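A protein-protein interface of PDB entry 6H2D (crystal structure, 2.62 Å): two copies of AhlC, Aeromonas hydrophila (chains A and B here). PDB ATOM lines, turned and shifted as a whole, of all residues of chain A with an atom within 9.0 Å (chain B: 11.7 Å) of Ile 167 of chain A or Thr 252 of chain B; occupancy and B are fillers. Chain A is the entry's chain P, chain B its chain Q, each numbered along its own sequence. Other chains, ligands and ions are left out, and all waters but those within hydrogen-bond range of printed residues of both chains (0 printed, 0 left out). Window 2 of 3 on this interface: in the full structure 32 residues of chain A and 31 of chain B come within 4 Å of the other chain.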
ATOM      1  N   LYS A 152     -30.889 -22.167 -11.900  1.00  0.00           N
ATOM      2  CA  LYS A 152     -29.529 -21.857 -11.461  1.00  0.00           C
ATOM      3  C   LYS A 152     -28.784 -23.161 -11.173  1.00  0.00           C
ATOM      4  O   LYS A 152     -27.734 -23.421 -11.767  1.00  0.00           O
ATOM      5  CB  LYS A 152     -29.492 -20.982 -10.206  1.00  0.00           C
ATOM      6  CG  LYS A 152     -28.098 -20.803  -9.622  1.00  0.00           C
ATOM      7  CD  LYS A 152     -28.009 -19.873  -8.440  1.00  0.00           C
ATOM      8  CE  LYS A 152     -26.571 -19.598  -8.046  1.00  0.00           C
ATOM      9  NZ  LYS A 152     -26.423 -18.300  -7.344  1.00  0.00           N
ATOM     10  N   LEU A 155     -28.160 -25.371 -14.280  1.00  0.00           N
ATOM     11  CA  LEU A 155     -27.165 -24.665 -15.057  1.00  0.00           C
ATOM     12  C   LEU A 155     -25.924 -24.412 -14.187  1.00  0.00           C
ATOM     13  O   LEU A 155     -25.743 -24.994 -13.100  1.00  0.00           O
ATOM     14  CB  LEU A 155     -27.783 -23.360 -15.573  1.00  0.00           C
ATOM     15  CG  LEU A 155     -28.970 -23.508 -16.527  1.00  0.00           C
ATOM     16  CD1 LEU A 155     -29.422 -22.148 -17.042  1.00  0.00           C
ATOM     17  CD2 LEU A 155     -28.635 -24.425 -17.697  1.00  0.00           C
ATOM     18  N   PRO A 164     -23.316 -18.735 -20.239  1.00  0.00           N
ATOM     19  CA  PRO A 164     -24.324 -18.247 -21.201  1.00  0.00           C
ATOM     20  C   PRO A 164     -25.742 -18.265 -20.594  1.00  0.00           C
ATOM     21  O   PRO A 164     -26.432 -17.233 -20.554  1.00  0.00           O
ATOM     22  CB  PRO A 164     -24.221 -19.153 -22.443  1.00  0.00           C
ATOM     23  CG  PRO A 164     -23.218 -20.240 -22.087  1.00  0.00           C
ATOM     24  CD  PRO A 164     -22.849 -20.067 -20.622  1.00  0.00           C
ATOM     25  N   GLY A 165     -26.167 -19.438 -20.111  1.00  0.00           N
ATOM     26  CA  GLY A 165     -27.429 -19.592 -19.397  1.00  0.00           C
ATOM     27  C   GLY A 165     -27.408 -18.846 -18.072  1.00  0.00           C
ATOM     28  O   GLY A 165     -28.300 -18.040 -17.791  1.00  0.00           O
ATOM     29  N   LEU A 166     -26.354 -19.100 -17.287  1.00  0.00           N
ATOM     30  CA  LEU A 166     -26.193 -18.585 -15.918  1.00  0.00           C
ATOM     31  C   LEU A 166     -26.153 -17.052 -15.898  1.00  0.00           C
ATOM     32  O   LEU A 166     -26.574 -16.454 -14.916  1.00  0.00           O
ATOM     33  CB  LEU A 166     -24.908 -19.156 -15.312  1.00  0.00           C
ATOM     34  CG  LEU A 166     -24.917 -20.660 -15.048  1.00  0.00           C
ATOM     35  CD1 LEU A 166     -23.511 -21.183 -14.794  1.00  0.00           C
ATOM     36  CD2 LEU A 166     -25.829 -20.998 -13.879  1.00  0.00           C
ATOM     37  N   ILE A 167     -25.627 -16.439 -16.970  1.00  0.00           N
ATOM     38  CA  ILE A 167     -25.547 -14.971 -17.105  1.00  0.00           C
ATOM     39  C   ILE A 167     -26.938 -14.392 -17.399  1.00  0.00           C
ATOM     40  O   ILE A 167     -27.338 -13.385 -16.810  1.00  0.00           O
ATOM     41  CB  ILE A 167     -24.505 -14.575 -18.171  1.00  0.00           C
ATOM     42  CG1 ILE A 167     -23.088 -14.551 -17.573  1.00  0.00           C
ATOM     43  CG2 ILE A 167     -24.886 -13.253 -18.840  1.00  0.00           C
ATOM     44  CD1 ILE A 167     -21.988 -14.994 -18.522  1.00  0.00           C
ATOM     45  N   ALA A 168     -27.684 -15.051 -18.289  1.00  0.00           N
ATOM     46  CA  ALA A 168     -29.031 -14.622 -18.674  1.00  0.00           C
ATOM     47  C   ALA A 168     -30.030 -14.727 -17.502  1.00  0.00           C
ATOM     48  O   ALA A 168     -31.118 -14.176 -17.564  1.00  0.00           O
ATOM     49  CB  ALA A 168     -29.479 -15.427 -19.873  1.00  0.00           C
ATOM     50  N   LEU A 169     -29.649 -15.411 -16.420  1.00  0.00           N
ATOM     51  CA  LEU A 169     -30.529 -15.691 -15.267  1.00  0.00           C
ATOM     52  C   LEU A 169     -30.172 -14.797 -14.062  1.00  0.00           C
ATOM     53  O   LEU A 169     -31.013 -14.577 -13.183  1.00  0.00           O
ATOM     54  CB  LEU A 169     -30.354 -17.183 -14.955  1.00  0.00           C
ATOM     55  CG  LEU A 169     -30.708 -17.650 -13.551  1.00  0.00           C
ATOM     56  CD1 LEU A 169     -32.206 -17.551 -13.340  1.00  0.00           C
ATOM     57  CD2 LEU A 169     -30.236 -19.073 -13.342  1.00  0.00           C
ATOM     58  N   ALA A 170     -28.936 -14.276 -14.026  1.00  0.00           N
ATOM     59  CA  ALA A 170     -28.314 -13.766 -12.796  1.00  0.00           C
ATOM     60  C   ALA A 170     -29.117 -12.606 -12.203  1.00  0.00           C
ATOM     61  O   ALA A 170     -29.361 -12.623 -11.004  1.00  0.00           O
ATOM     62  CB  ALA A 170     -26.887 -13.340 -13.033  1.00  0.00           C
ATOM     63  N   VAL A 171     -29.489 -11.607 -13.015  1.00  0.00           N
ATOM     64  CA  VAL A 171     -30.103 -10.348 -12.501  1.00  0.00           C
ATOM     65  C   VAL A 171     -31.534 -10.631 -12.006  1.00  0.00           C
ATOM     66  O   VAL A 171     -31.869 -10.314 -10.867  1.00  0.00           O
ATOM     67  CB  VAL A 171     -30.085  -9.208 -13.547  1.00  0.00           C
ATOM     68  CG1 VAL A 171     -30.786  -7.951 -13.035  1.00  0.00           C
ATOM     69  CG2 VAL A 171     -28.677  -8.851 -14.018  1.00  0.00           C
ATOM     70  N   THR A 172     -32.355 -11.213 -12.892  1.00  0.00           N
ATOM     71  CA  THR A 172     -33.673 -11.800 -12.623  1.00  0.00           C
ATOM     72  C   THR A 172     -33.722 -12.586 -11.299  1.00  0.00           C
ATOM     73  O   THR A 172     -34.663 -12.456 -10.540  1.00  0.00           O
ATOM     74  CB  THR A 172     -34.055 -12.764 -13.754  1.00  0.00           C
ATOM     75  OG1 THR A 172     -33.454 -12.273 -14.952  1.00  0.00           O
ATOM     76  CG2 THR A 172     -35.550 -12.915 -13.943  1.00  0.00           C
ATOM     77  N   LEU A 173     -32.745 -13.465 -11.068  1.00  0.00           N
ATOM     78  CA  LEU A 173     -32.623 -14.238  -9.810  1.00  0.00           C
ATOM     79  C   LEU A 173     -32.639 -13.274  -8.608  1.00  0.00           C
ATOM     80  O   LEU A 173     -33.558 -13.290  -7.785  1.00  0.00           O
ATOM     81  CB  LEU A 173     -31.336 -15.081  -9.875  1.00  0.00           C
ATOM     82  CG  LEU A 173     -30.976 -15.887  -8.625  1.00  0.00           C
ATOM     83  CD1 LEU A 173     -32.078 -16.868  -8.262  1.00  0.00           C
ATOM     84  CD2 LEU A 173     -29.667 -16.622  -8.821  1.00  0.00           C
ATOM     85  N   THR A 174     -31.624 -12.412  -8.530  1.00  0.00           N
ATOM     86  CA  THR A 174     -31.490 -11.430  -7.479  1.00  0.00           C
ATOM     87  C   THR A 174     -32.749 -10.550  -7.393  1.00  0.00           C
ATOM     88  O   THR A 174     -33.195 -10.202  -6.298  1.00  0.00           O
ATOM     89  CB  THR A 174     -30.244 -10.578  -7.737  1.00  0.00           C
ATOM     90  OG1 THR A 174     -29.186 -11.492  -8.037  1.00  0.00           O
ATOM     91  CG2 THR A 174     -29.872  -9.686  -6.577  1.00  0.00           C
ATOM     92  N   ARG B  61     -17.672  -5.830  -0.885  1.00  0.00           N
ATOM     93  CA  ARG B  61     -16.433  -6.314  -1.520  1.00  0.00           C
ATOM     94  C   ARG B  61     -16.522  -7.833  -1.766  1.00  0.00           C
ATOM     95  O   ARG B  61     -16.954  -8.316  -2.830  1.00  0.00           O
ATOM     96  CB  ARG B  61     -15.231  -5.992  -0.624  1.00  0.00           C
ATOM     97  CG  ARG B  61     -14.987  -4.503  -0.396  1.00  0.00           C
ATOM     98  CD  ARG B  61     -13.761  -4.197   0.461  1.00  0.00           C
ATOM     99  NE  ARG B  61     -13.571  -2.771   0.721  1.00  0.00           N
ATOM    100  CZ  ARG B  61     -12.960  -2.276   1.793  1.00  0.00           C
ATOM    101  NH1 ARG B  61     -12.261  -3.073   2.583  1.00  0.00           N
ATOM    102  NH2 ARG B  61     -13.077  -0.992   2.088  1.00  0.00           N
ATOM    103  N   THR B 224     -24.558 -20.317   1.934  1.00  0.00           N
ATOM    104  CA  THR B 224     -24.125 -19.440   0.843  1.00  0.00           C
ATOM    105  C   THR B 224     -22.610 -19.188   0.960  1.00  0.00           C
ATOM    106  O   THR B 224     -21.841 -19.460   0.042  1.00  0.00           O
ATOM    107  CB  THR B 224     -24.969 -18.157   0.848  1.00  0.00           C
ATOM    108  OG1 THR B 224     -26.345 -18.533   0.746  1.00  0.00           O
ATOM    109  CG2 THR B 224     -24.633 -17.208  -0.282  1.00  0.00           C
ATOM    110  N   LEU B 227     -20.915 -22.056  -0.269  1.00  0.00           N
ATOM    111  CA  LEU B 227     -21.057 -22.009  -1.723  1.00  0.00           C
ATOM    112  C   LEU B 227     -20.042 -21.023  -2.314  1.00  0.00           C
ATOM    113  O   LEU B 227     -19.361 -21.352  -3.297  1.00  0.00           O
ATOM    114  CB  LEU B 227     -22.477 -21.567  -2.106  1.00  0.00           C
ATOM    115  CG  LEU B 227     -23.587 -22.613  -1.989  1.00  0.00           C
ATOM    116  CD1 LEU B 227     -24.953 -21.948  -2.100  1.00  0.00           C
ATOM    117  CD2 LEU B 227     -23.442 -23.703  -3.043  1.00  0.00           C
ATOM    118  N   LEU B 228     -19.976 -19.821  -1.711  1.00  0.00           N
ATOM    119  CA  LEU B 228     -19.218 -18.670  -2.228  1.00  0.00           C
ATOM    120  C   LEU B 228     -17.722 -18.991  -2.246  1.00  0.00           C
ATOM    121  O   LEU B 228     -17.029 -18.585  -3.161  1.00  0.00           O
ATOM    122  CB  LEU B 228     -19.484 -17.443  -1.350  1.00  0.00           C
ATOM    123  CG  LEU B 228     -18.705 -16.185  -1.735  1.00  0.00           C
ATOM    124  CD1 LEU B 228     -18.988 -15.801  -3.175  1.00  0.00           C
ATOM    125  CD2 LEU B 228     -19.019 -15.012  -0.813  1.00  0.00           C
ATOM    126  N   GLY B 229     -17.268 -19.708  -1.211  1.00  0.00           N
ATOM    127  CA  GLY B 229     -15.876 -20.045  -0.988  1.00  0.00           C
ATOM    128  C   GLY B 229     -15.450 -21.208  -1.858  1.00  0.00           C
ATOM    129  O   GLY B 229     -14.277 -21.305  -2.253  1.00  0.00           O
ATOM    130  N   GLY B 230     -16.411 -22.093  -2.146  1.00  0.00           N
ATOM    131  CA  GLY B 230     -16.267 -23.062  -3.212  1.00  0.00           C
ATOM    132  C   GLY B 230     -15.984 -22.380  -4.547  1.00  0.00           C
ATOM    133  O   GLY B 230     -15.045 -22.753  -5.243  1.00  0.00           O
ATOM    134  N   ASP B 231     -16.780 -21.350  -4.877  1.00  0.00           N
ATOM    135  CA  ASP B 231     -16.746 -20.637  -6.181  1.00  0.00           C
ATOM    136  C   ASP B 231     -15.422 -19.888  -6.350  1.00  0.00           C
ATOM    137  O   ASP B 231     -14.796 -19.962  -7.406  1.00  0.00           O
ATOM    138  CB  ASP B 231     -17.920 -19.664  -6.320  1.00  0.00           C
ATOM    139  CG  ASP B 231     -19.263 -20.376  -6.412  1.00  0.00           C
ATOM    140  OD1 ASP B 231     -19.246 -21.620  -6.589  1.00  0.00           O
ATOM    141  OD2 ASP B 231     -20.317 -19.690  -6.310  1.00  0.00           O
ATOM    142  N   ILE B 232     -15.018 -19.180  -5.291  1.00  0.00           N
ATOM    143  CA  ILE B 232     -13.835 -18.326  -5.283  1.00  0.00           C
ATOM    144  C   ILE B 232     -12.572 -19.190  -5.415  1.00  0.00           C
ATOM    145  O   ILE B 232     -11.810 -19.028  -6.369  1.00  0.00           O
ATOM    146  CB  ILE B 232     -13.828 -17.447  -4.017  1.00  0.00           C
ATOM    147  CG1 ILE B 232     -14.742 -16.229  -4.182  1.00  0.00           C
ATOM    148  CG2 ILE B 232     -12.413 -17.039  -3.629  1.00  0.00           C
ATOM    149  CD1 ILE B 232     -15.092 -15.545  -2.874  1.00  0.00           C
ATOM    150  N   ALA B 233     -12.370 -20.110  -4.464  1.00  0.00           N
ATOM    151  CA  ALA B 233     -11.200 -20.996  -4.425  1.00  0.00           C
ATOM    152  C   ALA B 233     -10.914 -21.619  -5.808  1.00  0.00           C
ATOM    153  O   ALA B 233      -9.744 -21.803  -6.173  1.00  0.00           O
ATOM    154  CB  ALA B 233     -11.416 -22.048  -3.366  1.00  0.00           C
ATOM    155  N   ASN B 234     -11.972 -21.944  -6.571  1.00  0.00           N
ATOM    156  CA  ASN B 234     -11.861 -22.394  -7.974  1.00  0.00           C
ATOM    157  C   ASN B 234     -11.726 -21.176  -8.900  1.00  0.00           C
ATOM    158  O   ASN B 234     -10.630 -20.819  -9.321  1.00  0.00           O
ATOM    159  CB  ASN B 234     -13.070 -23.222  -8.422  1.00  0.00           C
ATOM    160  CG  ASN B 234     -13.457 -24.311  -7.444  1.00  0.00           C
ATOM    161  OD1 ASN B 234     -12.902 -24.369  -6.346  1.00  0.00           O
ATOM    162  ND2 ASN B 234     -14.404 -25.160  -7.829  1.00  0.00           N
ATOM    163  N   PHE B 250     -17.518 -18.704 -12.731  1.00  0.00           N
ATOM    164  CA  PHE B 250     -16.941 -18.972 -11.389  1.00  0.00           C
ATOM    165  C   PHE B 250     -16.876 -17.667 -10.599  1.00  0.00           C
ATOM    166  O   PHE B 250     -17.419 -17.585  -9.493  1.00  0.00           O
ATOM    167  CB  PHE B 250     -15.546 -19.594 -11.452  1.00  0.00           C
ATOM    168  CG  PHE B 250     -15.472 -21.099 -11.397  1.00  0.00           C
ATOM    169  CD1 PHE B 250     -16.606 -21.900 -11.387  1.00  0.00           C
ATOM    170  CD2 PHE B 250     -14.236 -21.727 -11.403  1.00  0.00           C
ATOM    171  CE1 PHE B 250     -16.504 -23.283 -11.346  1.00  0.00           C
ATOM    172  CE2 PHE B 250     -14.137 -23.109 -11.398  1.00  0.00           C
ATOM    173  CZ  PHE B 250     -15.273 -23.886 -11.367  1.00  0.00           C
ATOM    174  N   PHE B 251     -16.203 -16.660 -11.154  1.00  0.00           N
ATOM    175  CA  PHE B 251     -16.361 -15.340 -10.617  1.00  0.00           C
ATOM    176  C   PHE B 251     -17.850 -14.989 -10.720  1.00  0.00           C
ATOM    177  O   PHE B 251     -18.387 -14.270  -9.872  1.00  0.00           O
ATOM    178  CB  PHE B 251     -15.497 -14.317 -11.350  1.00  0.00           C
ATOM    179  CG  PHE B 251     -14.029 -14.340 -11.014  1.00  0.00           C
ATOM    180  CD1 PHE B 251     -13.129 -14.996 -11.843  1.00  0.00           C
ATOM    181  CD2 PHE B 251     -13.535 -13.656  -9.914  1.00  0.00           C
ATOM    182  CE1 PHE B 251     -11.772 -14.996 -11.557  1.00  0.00           C
ATOM    183  CE2 PHE B 251     -12.175 -13.650  -9.636  1.00  0.00           C
ATOM    184  CZ  PHE B 251     -11.297 -14.314 -10.461  1.00  0.00           C
ATOM    185  N   THR B 252     -18.503 -15.524 -11.763  1.00  0.00           N
ATOM    186  CA  THR B 252     -19.910 -15.228 -12.074  1.00  0.00           C
ATOM    187  C   THR B 252     -20.803 -15.837 -10.976  1.00  0.00           C
ATOM    188  O   THR B 252     -21.650 -15.151 -10.390  1.00  0.00           O
ATOM    189  CB  THR B 252     -20.235 -15.685 -13.507  1.00  0.00           C
ATOM    190  OG1 THR B 252     -19.167 -15.286 -14.371  1.00  0.00           O
ATOM    191  CG2 THR B 252     -21.535 -15.126 -14.048  1.00  0.00           C
ATOM    192  N   ALA B 253     -20.575 -17.124 -10.691  1.00  0.00           N
ATOM    193  CA  ALA B 253     -21.236 -17.881  -9.630  1.00  0.00           C
ATOM    194  C   ALA B 253     -21.050 -17.161  -8.288  1.00  0.00           C
ATOM    195  O   ALA B 253     -22.031 -16.829  -7.615  1.00  0.00           O
ATOM    196  CB  ALA B 253     -20.683 -19.291  -9.587  1.00  0.00           C
ATOM    197  N   ALA B 254     -19.779 -16.906  -7.935  1.00  0.00           N
ATOM    198  CA  ALA B 254     -19.391 -16.193  -6.712  1.00  0.00           C
ATOM    199  C   ALA B 254     -20.187 -14.893  -6.592  1.00  0.00           C
ATOM    200  O   ALA B 254     -20.619 -14.552  -5.526  1.00  0.00           O
ATOM    201  CB  ALA B 254     -17.907 -15.913  -6.707  1.00  0.00           C
ATOM    202  N   LEU B 255     -20.366 -14.186  -7.708  1.00  0.00           N
ATOM    203  CA  LEU B 255     -21.077 -12.926  -7.721  1.00  0.00           C
ATOM    204  C   LEU B 255     -22.552 -13.178  -7.390  1.00  0.00           C
ATOM    205  O   LEU B 255     -23.145 -12.429  -6.590  1.00  0.00           O
ATOM    206  CB  LEU B 255     -20.913 -12.275  -9.099  1.00  0.00           C
ATOM    207  CG  LEU B 255     -21.800 -11.061  -9.382  1.00  0.00           C
ATOM    208  CD1 LEU B 255     -21.298  -9.827  -8.630  1.00  0.00           C
ATOM    209  CD2 LEU B 255     -21.898 -10.802 -10.883  1.00  0.00           C
ATOM    210  N   THR B 256     -23.144 -14.221  -8.002  1.00  0.00           N
ATOM    211  CA  THR B 256     -24.582 -14.523  -7.795  1.00  0.00           C
ATOM    212  C   THR B 256     -24.804 -15.005  -6.351  1.00  0.00           C
ATOM    213  O   THR B 256     -25.856 -14.748  -5.775  1.00  0.00           O
ATOM    214  CB  THR B 256     -25.155 -15.487  -8.850  1.00  0.00           C
ATOM    215  OG1 THR B 256     -24.524 -16.762  -8.774  1.00  0.00           O
ATOM    216  CG2 THR B 256     -25.026 -14.957 -10.262  1.00  0.00           C
ATOM    217  N   GLU B 257     -23.791 -15.648  -5.760  1.00  0.00           N
ATOM    218  CA  GLU B 257     -23.843 -16.055  -4.368  1.00  0.00           C
ATOM    219  C   GLU B 257     -23.683 -14.858  -3.409  1.00  0.00           C
ATOM    220  O   GLU B 257     -24.288 -14.886  -2.337  1.00  0.00           O
ATOM    221  CB  GLU B 257     -22.780 -17.108  -4.053  1.00  0.00           C
ATOM    222  CG  GLU B 257     -23.038 -18.472  -4.675  1.00  0.00           C
ATOM    223  CD  GLU B 257     -24.415 -19.081  -4.476  1.00  0.00           C
ATOM    224  OE1 GLU B 257     -25.053 -18.805  -3.443  1.00  0.00           O
ATOM    225  OE2 GLU B 257     -24.847 -19.835  -5.368  1.00  0.00           O
ATOM    226  N   VAL B 258     -22.867 -13.843  -3.729  1.00  0.00           N
ATOM    227  CA  VAL B 258     -22.696 -12.724  -2.760  1.00  0.00           C
ATOM    228  C   VAL B 258     -23.944 -11.853  -2.828  1.00  0.00           C
ATOM    229  O   VAL B 258     -24.238 -11.165  -1.879  1.00  0.00           O
ATOM    230  CB  VAL B 258     -21.449 -11.826  -2.945  1.00  0.00           C
ATOM    231  CG1 VAL B 258     -20.178 -12.608  -3.259  1.00  0.00           C
ATOM    232  CG2 VAL B 258     -21.678 -10.720  -3.967  1.00  0.00           C
ATOM    233  N   ARG B 259     -24.624 -11.863  -3.978  1.00  0.00           N
ATOM    234  CA  ARG B 259     -25.839 -11.077  -4.159  1.00  0.00           C
ATOM    235  C   ARG B 259     -27.008 -11.774  -3.428  1.00  0.00           C
ATOM    236  O   ARG B 259     -27.943 -11.091  -2.988  1.00  0.00           O
ATOM    237  CB  ARG B 259     -26.059 -10.817  -5.656  1.00  0.00           C
ATOM    238  CG  ARG B 259     -24.935 -10.023  -6.316  1.00  0.00           C
ATOM    239  CD  ARG B 259     -25.414  -8.994  -7.327  1.00  0.00           C
ATOM    240  NE  ARG B 259     -26.089  -9.621  -8.459  1.00  0.00           N
ATOM    241  CZ  ARG B 259     -26.696  -8.969  -9.449  1.00  0.00           C
ATOM    242  NH1 ARG B 259     -26.616  -7.650  -9.520  1.00  0.00           N
ATOM    243  NH2 ARG B 259     -27.394  -9.639 -10.357  1.00  0.00           N
ATOM    244  N   THR B 260     -26.934 -13.113  -3.261  1.00  0.00           N
ATOM    245  CA  THR B 260     -27.880 -13.899  -2.397  1.00  0.00           C
ATOM    246  C   THR B 260     -27.639 -13.621  -0.908  1.00  0.00           C
ATOM    247  O   THR B 260     -28.543 -13.736  -0.108  1.00  0.00           O
ATOM    248  CB  THR B 260     -27.759 -15.428  -2.533  1.00  0.00           C
ATOM    249  OG1 THR B 260     -27.809 -15.869  -3.888  1.00  0.00           O
ATOM    250  CG2 THR B 260     -28.861 -16.147  -1.784  1.00  0.00           C
ATOM    251  N   LEU B 261     -26.386 -13.321  -0.566  1.00  0.00           N
ATOM    252  CA  LEU B 261     -25.929 -13.117   0.785  1.00  0.00           C
ATOM    253  C   LEU B 261     -26.257 -11.685   1.236  1.00  0.00           C
ATOM    254  O   LEU B 261     -26.341 -11.433   2.425  1.00  0.00           O
ATOM    255  CB  LEU B 261     -24.425 -13.410   0.795  1.00  0.00           C
ATOM    256  CG  LEU B 261     -23.753 -13.535   2.161  1.00  0.00           C
ATOM    257  CD1 LEU B 261     -24.125 -14.842   2.846  1.00  0.00           C
ATOM    258  CD2 LEU B 261     -22.239 -13.430   2.025  1.00  0.00           C
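The side-chain hydroxyl of Thr 256 of chain B lies within hydrogen-bond range of the side-chain amino group of Lys 152 of chain A, 2.8 Å away. OE2 of Glu 257 of chain B is in salt-bridge range of NZ of Lys 152 of chain A (3.0 Å). OG1 of Thr 174 of chain A sits at hydrogen-bond distance from NH2 of Arg 259 of chain B (3.5 Å).
The backbone carbonyl oxygen (O) of Ala 170 of chain A lies within hydrogen-bond range of the side-chain hydroxyl (OG1) of Thr 174 of chain A (3.2 Å). O of Ala 253 of chain B lies within hydrogen-bond range of OG1 of Thr 256 of chain B (2.8 Å). The side-chain hydroxyl (OG1) of Thr 260 of chain B lies within hydrogen-bond range of the backbone carbonyl oxygen (O) of Thr 256 of chain B.
Ile 167 of chain A touches Thr 252 of chain B (CG1 to CG2, 3.9 Å). CB of Ala 170 of chain A touches CG2 of Thr 256 of chain B, at 3.7 Å. Ala 170 of chain A touches Arg 259 of chain B. Val 171 of chain A touches Arg 259 of chain B.
Of chain B, only Thr 252 (3.9 Å) comes within 4 Å of Ile 167 of chain A. Of chain A, only Ile 167 comes within 4 Å of Thr 252 of chain B. No residue of chain B comes within 4 Å of Pro 164 of chain A. No residue of chain B comes within 4 Å of Leu 166 of chain A. Of the printed residues of chain B, Val 171 of chain A touches Arg 259. Printed residues of chain A within 4 Å of Thr 256 of chain B: Lys 152 and Ala 170. Of the printed residues of chain A, Arg 259 of chain B touches Ala 170, Val 171 and Thr 174. Of the printed residues of chain B, Thr 174 of chain A touches Arg 259 (3.5 Å). The nearest residue of chain B that does not touch Ile 167 of chain A is Thr 256 of chain B (6.9 Å). The nearest residue of chain A that does not touch Thr 252 of chain B is Leu 166 of chain A (5.3 Å).
Of the 13 printed residues of chain A, 5 touch a printed residue of chain B. Of the 22 printed residues of chain B, 4 touch a printed residue of chain A. Among the printed residues, 7 pairs touch across the chains. Among the printed residues, Asp or Glu carboxylates within 4 Å of a Lys or Arg side-chain nitrogen of the other chain: Lys 152 of chain A with Glu 257 of chain B (3.0 Å).
No position is printed for both chains. Of the 7 pairs that touch across the chains among the printed residues, none has its exchanged pair printed and touching as well.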
